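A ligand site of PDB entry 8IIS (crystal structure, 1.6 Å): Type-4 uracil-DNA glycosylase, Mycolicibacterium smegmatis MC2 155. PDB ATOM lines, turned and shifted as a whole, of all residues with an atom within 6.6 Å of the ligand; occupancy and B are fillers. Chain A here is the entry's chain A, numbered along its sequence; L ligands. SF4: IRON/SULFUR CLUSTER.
SG of Cys 32 binds FE3 of the ligand.
The backbone NH (N) of Cys 35 sits close to a sulfur (S1) of the ligand (3.6 Å).
The indole nitrogen (NE1) of Trp 131 sits close to a sulfur (S2) of the ligand (3.7 Å).
A sulfur (S1) of the ligand lies close to the backbone NH of Gly 34 (3.6 Å).
An iron atom (FE2) of the ligand is bound by the side-chain sulfur (SG) of Cys 35 (2.3 Å).
N of Lys 102 lies close to S3 of the ligand (3.7 Å).
SG of Cys 128 binds FE1 of the ligand (2.3 Å).
A sulfur (S3) of the ligand sits close to the backbone NH (N) of His 103 (3.6 Å).
FE4 of the ligand is bound by ND1 of His 103 (2.3 Å).
SG of Cys 32 sits close to N of Gly 34, 3.3 Å away.
The backbone NH of Ala 44 is in hydrogen-bond range of a ring nitrogen (NE2) of His 103, at 3.2 Å.
The side-chain sulfur (SG) of Cys 128 lies close to the backbone NH (N) of Lys 102 (3.5 Å).
The backbone carbonyl oxygen of Ala 127 sits at hydrogen-bond distance from the backbone NH of Ala 12 (2.8 Å).
SG of Cys 35 lies close to N of Leu 37 (3.5 Å).
The side-chain sulfur (SG) of Cys 32 lies close to the indole nitrogen (NE1) of Trp 131 (3.3 Å).
Residues that only touch the ligand: Tyr 38 (3.8 Å), Ala 127 (3.9 Å) and Ala 12 (3.9 Å).
Hydrophobic or aromatic side chains that line the ligand: Ala 12, Tyr 38, His 103 and Trp 131.
Within 4 Å of the ligand: Ala 12, Cys 32, Gly 34, Cys 35, Tyr 38, Lys 102, His 103, Ala 127, Cys 128 and Trp 131.
The nearest printed residue that does not touch the ligand is Arg 33 (4.02 Å).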
ATOM      1  N   GLY A  11      26.956  15.787  27.886  1.00  0.00           N
ATOM      2  CA  GLY A  11      26.257  15.496  26.623  1.00  0.00           C
ATOM      3  C   GLY A  11      26.683  16.372  25.458  1.00  0.00           C
ATOM      4  O   GLY A  11      27.874  16.692  25.268  1.00  0.00           O
ATOM      5  N   ALA A  12      25.681  16.767  24.659  1.00  0.00           N
ATOM      6  CA  ALA A  12      25.889  17.626  23.477  1.00  0.00           C
ATOM      7  C   ALA A  12      25.961  19.096  23.800  1.00  0.00           C
ATOM      8  O   ALA A  12      26.154  19.876  22.875  1.00  0.00           O
ATOM      9  CB  ALA A  12      24.719  17.451  22.499  1.00  0.00           C
ATOM     10  N   PHE A  15      28.354  21.575  22.140  1.00  0.00           N
ATOM     11  CA  PHE A  15      28.343  21.611  20.694  1.00  0.00           C
ATOM     12  C   PHE A  15      27.212  22.464  20.170  1.00  0.00           C
ATOM     13  O   PHE A  15      27.240  22.772  18.984  1.00  0.00           O
ATOM     14  CB  PHE A  15      28.217  20.167  20.151  1.00  0.00           C
ATOM     15  CG  PHE A  15      29.422  19.302  20.457  1.00  0.00           C
ATOM     16  CD1 PHE A  15      30.577  19.447  19.674  1.00  0.00           C
ATOM     17  CD2 PHE A  15      29.389  18.388  21.501  1.00  0.00           C
ATOM     18  CE1 PHE A  15      31.717  18.627  19.934  1.00  0.00           C
ATOM     19  CE2 PHE A  15      30.558  17.592  21.828  1.00  0.00           C
ATOM     20  CZ  PHE A  15      31.672  17.718  21.032  1.00  0.00           C
ATOM     21  N   ALA A  29      25.283  20.576  14.456  1.00  0.00           N
ATOM     22  CA  ALA A  29      25.037  19.187  14.855  1.00  0.00           C
ATOM     23  C   ALA A  29      25.884  18.208  14.058  1.00  0.00           C
ATOM     24  O   ALA A  29      26.219  17.118  14.541  1.00  0.00           O
ATOM     25  CB  ALA A  29      23.521  18.872  14.733  1.00  0.00           C
ATOM     26  N   CYS A  32      28.724  17.341  16.117  1.00  0.00           N
ATOM     27  CA  CYS A  32      28.521  16.921  17.500  1.00  0.00           C
ATOM     28  C   CYS A  32      29.192  15.575  17.805  1.00  0.00           C
ATOM     29  O   CYS A  32      29.114  14.639  17.003  1.00  0.00           O
ATOM     30  CB  CYS A  32      26.988  16.836  17.744  1.00  0.00           C
ATOM     31  SG  CYS A  32      26.583  16.430  19.466  1.00  0.00           S
ATOM     32  N   ARG A  33      29.822  15.479  18.973  1.00  0.00           N
ATOM     33  CA  ARG A  33      30.364  14.222  19.492  1.00  0.00           C
ATOM     34  C   ARG A  33      29.815  13.962  20.891  1.00  0.00           C
ATOM     35  O   ARG A  33      30.439  13.279  21.688  1.00  0.00           O
ATOM     36  CB  ARG A  33      31.917  14.248  19.526  1.00  0.00           C
ATOM     37  CG  ARG A  33      32.557  14.544  18.174  1.00  0.00           C
ATOM     38  CD  ARG A  33      34.117  14.330  18.238  1.00  0.00           C
ATOM     39  NE  ARG A  33      34.678  15.006  19.421  1.00  0.00           N
ATOM     40  CZ  ARG A  33      34.881  16.301  19.437  1.00  0.00           C
ATOM     41  NH1 ARG A  33      34.539  17.037  18.394  1.00  0.00           N
ATOM     42  NH2 ARG A  33      35.364  16.885  20.519  1.00  0.00           N
ATOM     43  N   GLY A  34      28.594  14.456  21.153  1.00  0.00           N
ATOM     44  CA  GLY A  34      27.957  14.444  22.473  1.00  0.00           C
ATOM     45  C   GLY A  34      27.717  13.075  23.086  1.00  0.00           C
ATOM     46  O   GLY A  34      27.538  12.998  24.314  1.00  0.00           O
ATOM     47  N   CYS A  35      27.694  12.030  22.271  1.00  0.00           N
ATOM     48  CA  CYS A  35      27.622  10.625  22.738  1.00  0.00           C
ATOM     49  C   CYS A  35      28.366   9.814  21.704  1.00  0.00           C
ATOM     50  O   CYS A  35      29.004  10.379  20.797  1.00  0.00           O
ATOM     51  CB  CYS A  35      26.162  10.214  22.977  1.00  0.00           C
ATOM     52  SG  CYS A  35      25.203   9.876  21.422  1.00  0.00           S
ATOM     53  N   GLY A  36      28.302   8.482  21.823  1.00  0.00           N
ATOM     54  CA  GLY A  36      29.102   7.720  20.871  1.00  0.00           C
ATOM     55  C   GLY A  36      28.464   7.488  19.514  1.00  0.00           C
ATOM     56  O   GLY A  36      29.113   6.935  18.635  1.00  0.00           O
ATOM     57  N   LEU A  37      27.198   7.871  19.328  1.00  0.00           N
ATOM     58  CA  LEU A  37      26.486   7.451  18.107  1.00  0.00           C
ATOM     59  C   LEU A  37      27.023   8.105  16.844  1.00  0.00           C
ATOM     60  O   LEU A  37      26.745   7.623  15.739  1.00  0.00           O
ATOM     61  CB  LEU A  37      24.986   7.778  18.277  1.00  0.00           C
ATOM     62  CG  LEU A  37      24.360   6.999  19.451  1.00  0.00           C
ATOM     63  CD1 LEU A  37      22.859   7.369  19.523  1.00  0.00           C
ATOM     64  CD2 LEU A  37      24.521   5.458  19.200  1.00  0.00           C
ATOM     65  N   TYR A  38      27.787   9.207  16.957  1.00  0.00           N
ATOM     66  CA  TYR A  38      28.272   9.857  15.744  1.00  0.00           C
ATOM     67  C   TYR A  38      29.279   8.972  15.018  1.00  0.00           C
ATOM     68  O   TYR A  38      29.466   9.136  13.817  1.00  0.00           O
ATOM     69  CB  TYR A  38      28.925  11.224  16.073  1.00  0.00           C
ATOM     70  CG  TYR A  38      30.300  11.089  16.688  1.00  0.00           C
ATOM     71  CD1 TYR A  38      30.438  10.863  18.052  1.00  0.00           C
ATOM     72  CD2 TYR A  38      31.428  11.143  15.892  1.00  0.00           C
ATOM     73  CE1 TYR A  38      31.708  10.728  18.616  1.00  0.00           C
ATOM     74  CE2 TYR A  38      32.699  10.988  16.436  1.00  0.00           C
ATOM     75  CZ  TYR A  38      32.807  10.783  17.799  1.00  0.00           C
ATOM     76  OH  TYR A  38      34.056  10.622  18.378  1.00  0.00           O
ATOM     77  N   ARG A  39      29.915   8.058  15.722  1.00  0.00           N
ATOM     78  CA  ARG A  39      31.026   7.321  15.055  1.00  0.00           C
ATOM     79  C   ARG A  39      30.559   6.436  13.896  1.00  0.00           C
ATOM     80  O   ARG A  39      31.148   6.520  12.827  1.00  0.00           O
ATOM     81  CB  ARG A  39      31.800   6.473  16.058  1.00  0.00           C
ATOM     82  CG  ARG A  39      32.483   7.291  17.150  1.00  0.00           C
ATOM     83  CD  ARG A  39      32.988   6.377  18.247  1.00  0.00           C
ATOM     84  NE  ARG A  39      31.877   5.740  18.939  1.00  0.00           N
ATOM     85  CZ  ARG A  39      31.854   5.448  20.225  1.00  0.00           C
ATOM     86  N   ALA A  44      24.920  13.315  11.015  1.00  0.00           N
ATOM     87  CA  ALA A  44      23.806  13.751  11.856  1.00  0.00           C
ATOM     88  C   ALA A  44      22.626  14.097  10.963  1.00  0.00           C
ATOM     89  O   ALA A  44      22.799  14.556   9.815  1.00  0.00           O
ATOM     90  CB  ALA A  44      24.233  14.982  12.663  1.00  0.00           C
ATOM     91  N   ALA A 100      14.492  12.396  18.668  1.00  0.00           N
ATOM     92  CA  ALA A 100      15.084  12.605  19.996  1.00  0.00           C
ATOM     93  C   ALA A 100      16.589  12.511  19.957  1.00  0.00           C
ATOM     94  O   ALA A 100      17.268  13.229  20.678  1.00  0.00           O
ATOM     95  CB  ALA A 100      14.470  11.590  20.966  1.00  0.00           C
ATOM     96  N   VAL A 101      17.111  11.586  19.150  1.00  0.00           N
ATOM     97  CA  VAL A 101      18.579  11.521  18.928  1.00  0.00           C
ATOM     98  C   VAL A 101      18.834  11.751  17.435  1.00  0.00           C
ATOM     99  O   VAL A 101      17.952  11.419  16.649  1.00  0.00           O
ATOM    100  CB  VAL A 101      19.283  10.263  19.452  1.00  0.00           C
ATOM    101  CG1 VAL A 101      18.965  10.020  20.927  1.00  0.00           C
ATOM    102  CG2 VAL A 101      18.977   9.036  18.645  1.00  0.00           C
ATOM    103  N   LYS A 102      20.001  12.268  17.098  1.00  0.00           N
ATOM    104  CA  LYS A 102      20.243  12.725  15.712  1.00  0.00           C
ATOM    105  C   LYS A 102      21.237  11.878  14.931  1.00  0.00           C
ATOM    106  O   LYS A 102      21.461  12.187  13.788  1.00  0.00           O
ATOM    107  CB  LYS A 102      20.557  14.222  15.803  1.00  0.00           C
ATOM    108  CG  LYS A 102      19.277  14.938  16.215  1.00  0.00           C
ATOM    109  CD  LYS A 102      19.361  16.392  16.525  1.00  0.00           C
ATOM    110  CE  LYS A 102      17.996  17.034  16.375  1.00  0.00           C
ATOM    111  NZ  LYS A 102      17.046  16.636  17.448  1.00  0.00           N
ATOM    112  N   HIS A 103      21.699  10.799  15.542  1.00  0.00           N
ATOM    113  CA  HIS A 103      22.557   9.843  14.811  1.00  0.00           C
ATOM    114  C   HIS A 103      21.924   8.451  14.904  1.00  0.00           C
ATOM    115  O   HIS A 103      21.493   8.082  15.972  1.00  0.00           O
ATOM    116  CB  HIS A 103      23.998   9.789  15.295  1.00  0.00           C
ATOM    117  CG  HIS A 103      24.877  10.858  14.745  1.00  0.00           C
ATOM    118  ND1 HIS A 103      25.204  11.957  15.469  1.00  0.00           N
ATOM    119  CD2 HIS A 103      25.529  10.988  13.587  1.00  0.00           C
ATOM    120  CE1 HIS A 103      25.999  12.747  14.791  1.00  0.00           C
ATOM    121  NE2 HIS A 103      26.227  12.164  13.649  1.00  0.00           N
ATOM    122  N   PHE A 104      21.877   7.776  13.781  1.00  0.00           N
ATOM    123  CA  PHE A 104      21.311   6.417  13.691  1.00  0.00           C
ATOM    124  C   PHE A 104      22.175   5.438  14.461  1.00  0.00           C
ATOM    125  O   PHE A 104      23.384   5.352  14.242  1.00  0.00           O
ATOM    126  CB  PHE A 104      21.270   6.090  12.186  1.00  0.00           C
ATOM    127  CG  PHE A 104      20.744   4.724  11.813  1.00  0.00           C
ATOM    128  CD1 PHE A 104      19.649   4.161  12.474  1.00  0.00           C
ATOM    129  CD2 PHE A 104      21.322   4.050  10.705  1.00  0.00           C
ATOM    130  CE1 PHE A 104      19.148   2.888  12.062  1.00  0.00           C
ATOM    131  CE2 PHE A 104      20.821   2.807  10.324  1.00  0.00           C
ATOM    132  CZ  PHE A 104      19.714   2.241  10.978  1.00  0.00           C
ATOM    133  N   GLU A 124      21.974   8.221  26.064  1.00  0.00           N
ATOM    134  CA  GLU A 124      22.066   8.896  24.761  1.00  0.00           C
ATOM    135  C   GLU A 124      20.948   9.923  24.549  1.00  0.00           C
ATOM    136  O   GLU A 124      21.209  11.005  24.011  1.00  0.00           O
ATOM    137  CB  GLU A 124      22.042   7.847  23.620  1.00  0.00           C
ATOM    138  CG  GLU A 124      23.404   7.108  23.600  1.00  0.00           C
ATOM    139  CD  GLU A 124      23.335   5.704  23.002  1.00  0.00           C
ATOM    140  OE1 GLU A 124      22.226   5.117  22.806  1.00  0.00           O
ATOM    141  OE2 GLU A 124      24.426   5.139  22.734  1.00  0.00           O
ATOM    142  N   ALA A 127      21.858  12.909  26.507  1.00  0.00           N
ATOM    143  CA  ALA A 127      23.020  13.573  25.897  1.00  0.00           C
ATOM    144  C   ALA A 127      22.604  14.431  24.700  1.00  0.00           C
ATOM    145  O   ALA A 127      23.166  15.485  24.476  1.00  0.00           O
ATOM    146  CB  ALA A 127      24.055  12.526  25.439  1.00  0.00           C
ATOM    147  N   CYS A 128      21.628  13.941  23.904  1.00  0.00           N
ATOM    148  CA  CYS A 128      21.234  14.651  22.691  1.00  0.00           C
ATOM    149  C   CYS A 128      20.186  15.712  22.962  1.00  0.00           C
ATOM    150  O   CYS A 128      19.920  16.583  22.085  1.00  0.00           O
ATOM    151  CB  CYS A 128      20.714  13.605  21.691  1.00  0.00           C
ATOM    152  SG  CYS A 128      20.882  14.165  19.915  1.00  0.00           S
ATOM    153  N   ARG A 129      19.567  15.657  24.128  1.00  0.00           N
ATOM    154  CA  ARG A 129      18.431  16.574  24.415  1.00  0.00           C
ATOM    155  C   ARG A 129      18.744  18.051  24.196  1.00  0.00           C
ATOM    156  O   ARG A 129      17.827  18.769  23.843  1.00  0.00           O
ATOM    157  CB  ARG A 129      17.780  16.269  25.786  1.00  0.00           C
ATOM    158  CG  ARG A 129      16.308  16.637  25.879  1.00  0.00           C
ATOM    159  CD  ARG A 129      15.644  15.982  27.062  1.00  0.00           C
ATOM    160  NE  ARG A 129      16.416  16.149  28.280  1.00  0.00           N
ATOM    161  CZ  ARG A 129      16.203  15.488  29.404  1.00  0.00           C
ATOM    162  NH1 ARG A 129      15.213  14.611  29.481  1.00  0.00           N
ATOM    163  NH2 ARG A 129      16.979  15.703  30.451  1.00  0.00           N
ATOM    164  N   TRP A 131      20.018  19.435  21.749  1.00  0.00           N
ATOM    165  CA  TRP A 131      19.593  19.806  20.397  1.00  0.00           C
ATOM    166  C   TRP A 131      18.087  19.966  20.345  1.00  0.00           C
ATOM    167  O   TRP A 131      17.565  20.906  19.707  1.00  0.00           O
ATOM    168  CB  TRP A 131      20.021  18.734  19.376  1.00  0.00           C
ATOM    169  CG  TRP A 131      21.518  18.688  19.196  1.00  0.00           C
ATOM    170  CD1 TRP A 131      22.383  17.631  19.506  1.00  0.00           C
ATOM    171  CD2 TRP A 131      22.340  19.743  18.658  1.00  0.00           C
ATOM    172  NE1 TRP A 131      23.676  17.997  19.218  1.00  0.00           N
ATOM    173  CE2 TRP A 131      23.683  19.267  18.681  1.00  0.00           C
ATOM    174  CE3 TRP A 131      22.074  21.038  18.170  1.00  0.00           C
ATOM    175  CZ2 TRP A 131      24.766  20.062  18.238  1.00  0.00           C
ATOM    176  CZ3 TRP A 131      23.147  21.817  17.722  1.00  0.00           C
ATOM    177  CH2 TRP A 131      24.484  21.329  17.756  1.00  0.00           C
HETATM  178 FE1  SF4 L   1      22.980  13.498  19.449  1.00  0.00          FE
HETATM  179 FE2  SF4 L   1      24.985  11.842  20.250  1.00  0.00          FE
HETATM  180 FE3  SF4 L   1      25.513  14.374  19.354  1.00  0.00          FE
HETATM  181 FE4  SF4 L   1      24.710  12.487  17.670  1.00  0.00          FE
HETATM  182  S1  SF4 L   1      26.665  12.503  18.864  1.00  0.00           S
HETATM  183  S2  SF4 L   1      23.911  14.640  17.731  1.00  0.00           S
HETATM  184  S3  SF4 L   1      23.171  11.329  18.836  1.00  0.00           S
HETATM  185  S4  SF4 L   1      24.392  13.775  21.247  1.00  0.00           S
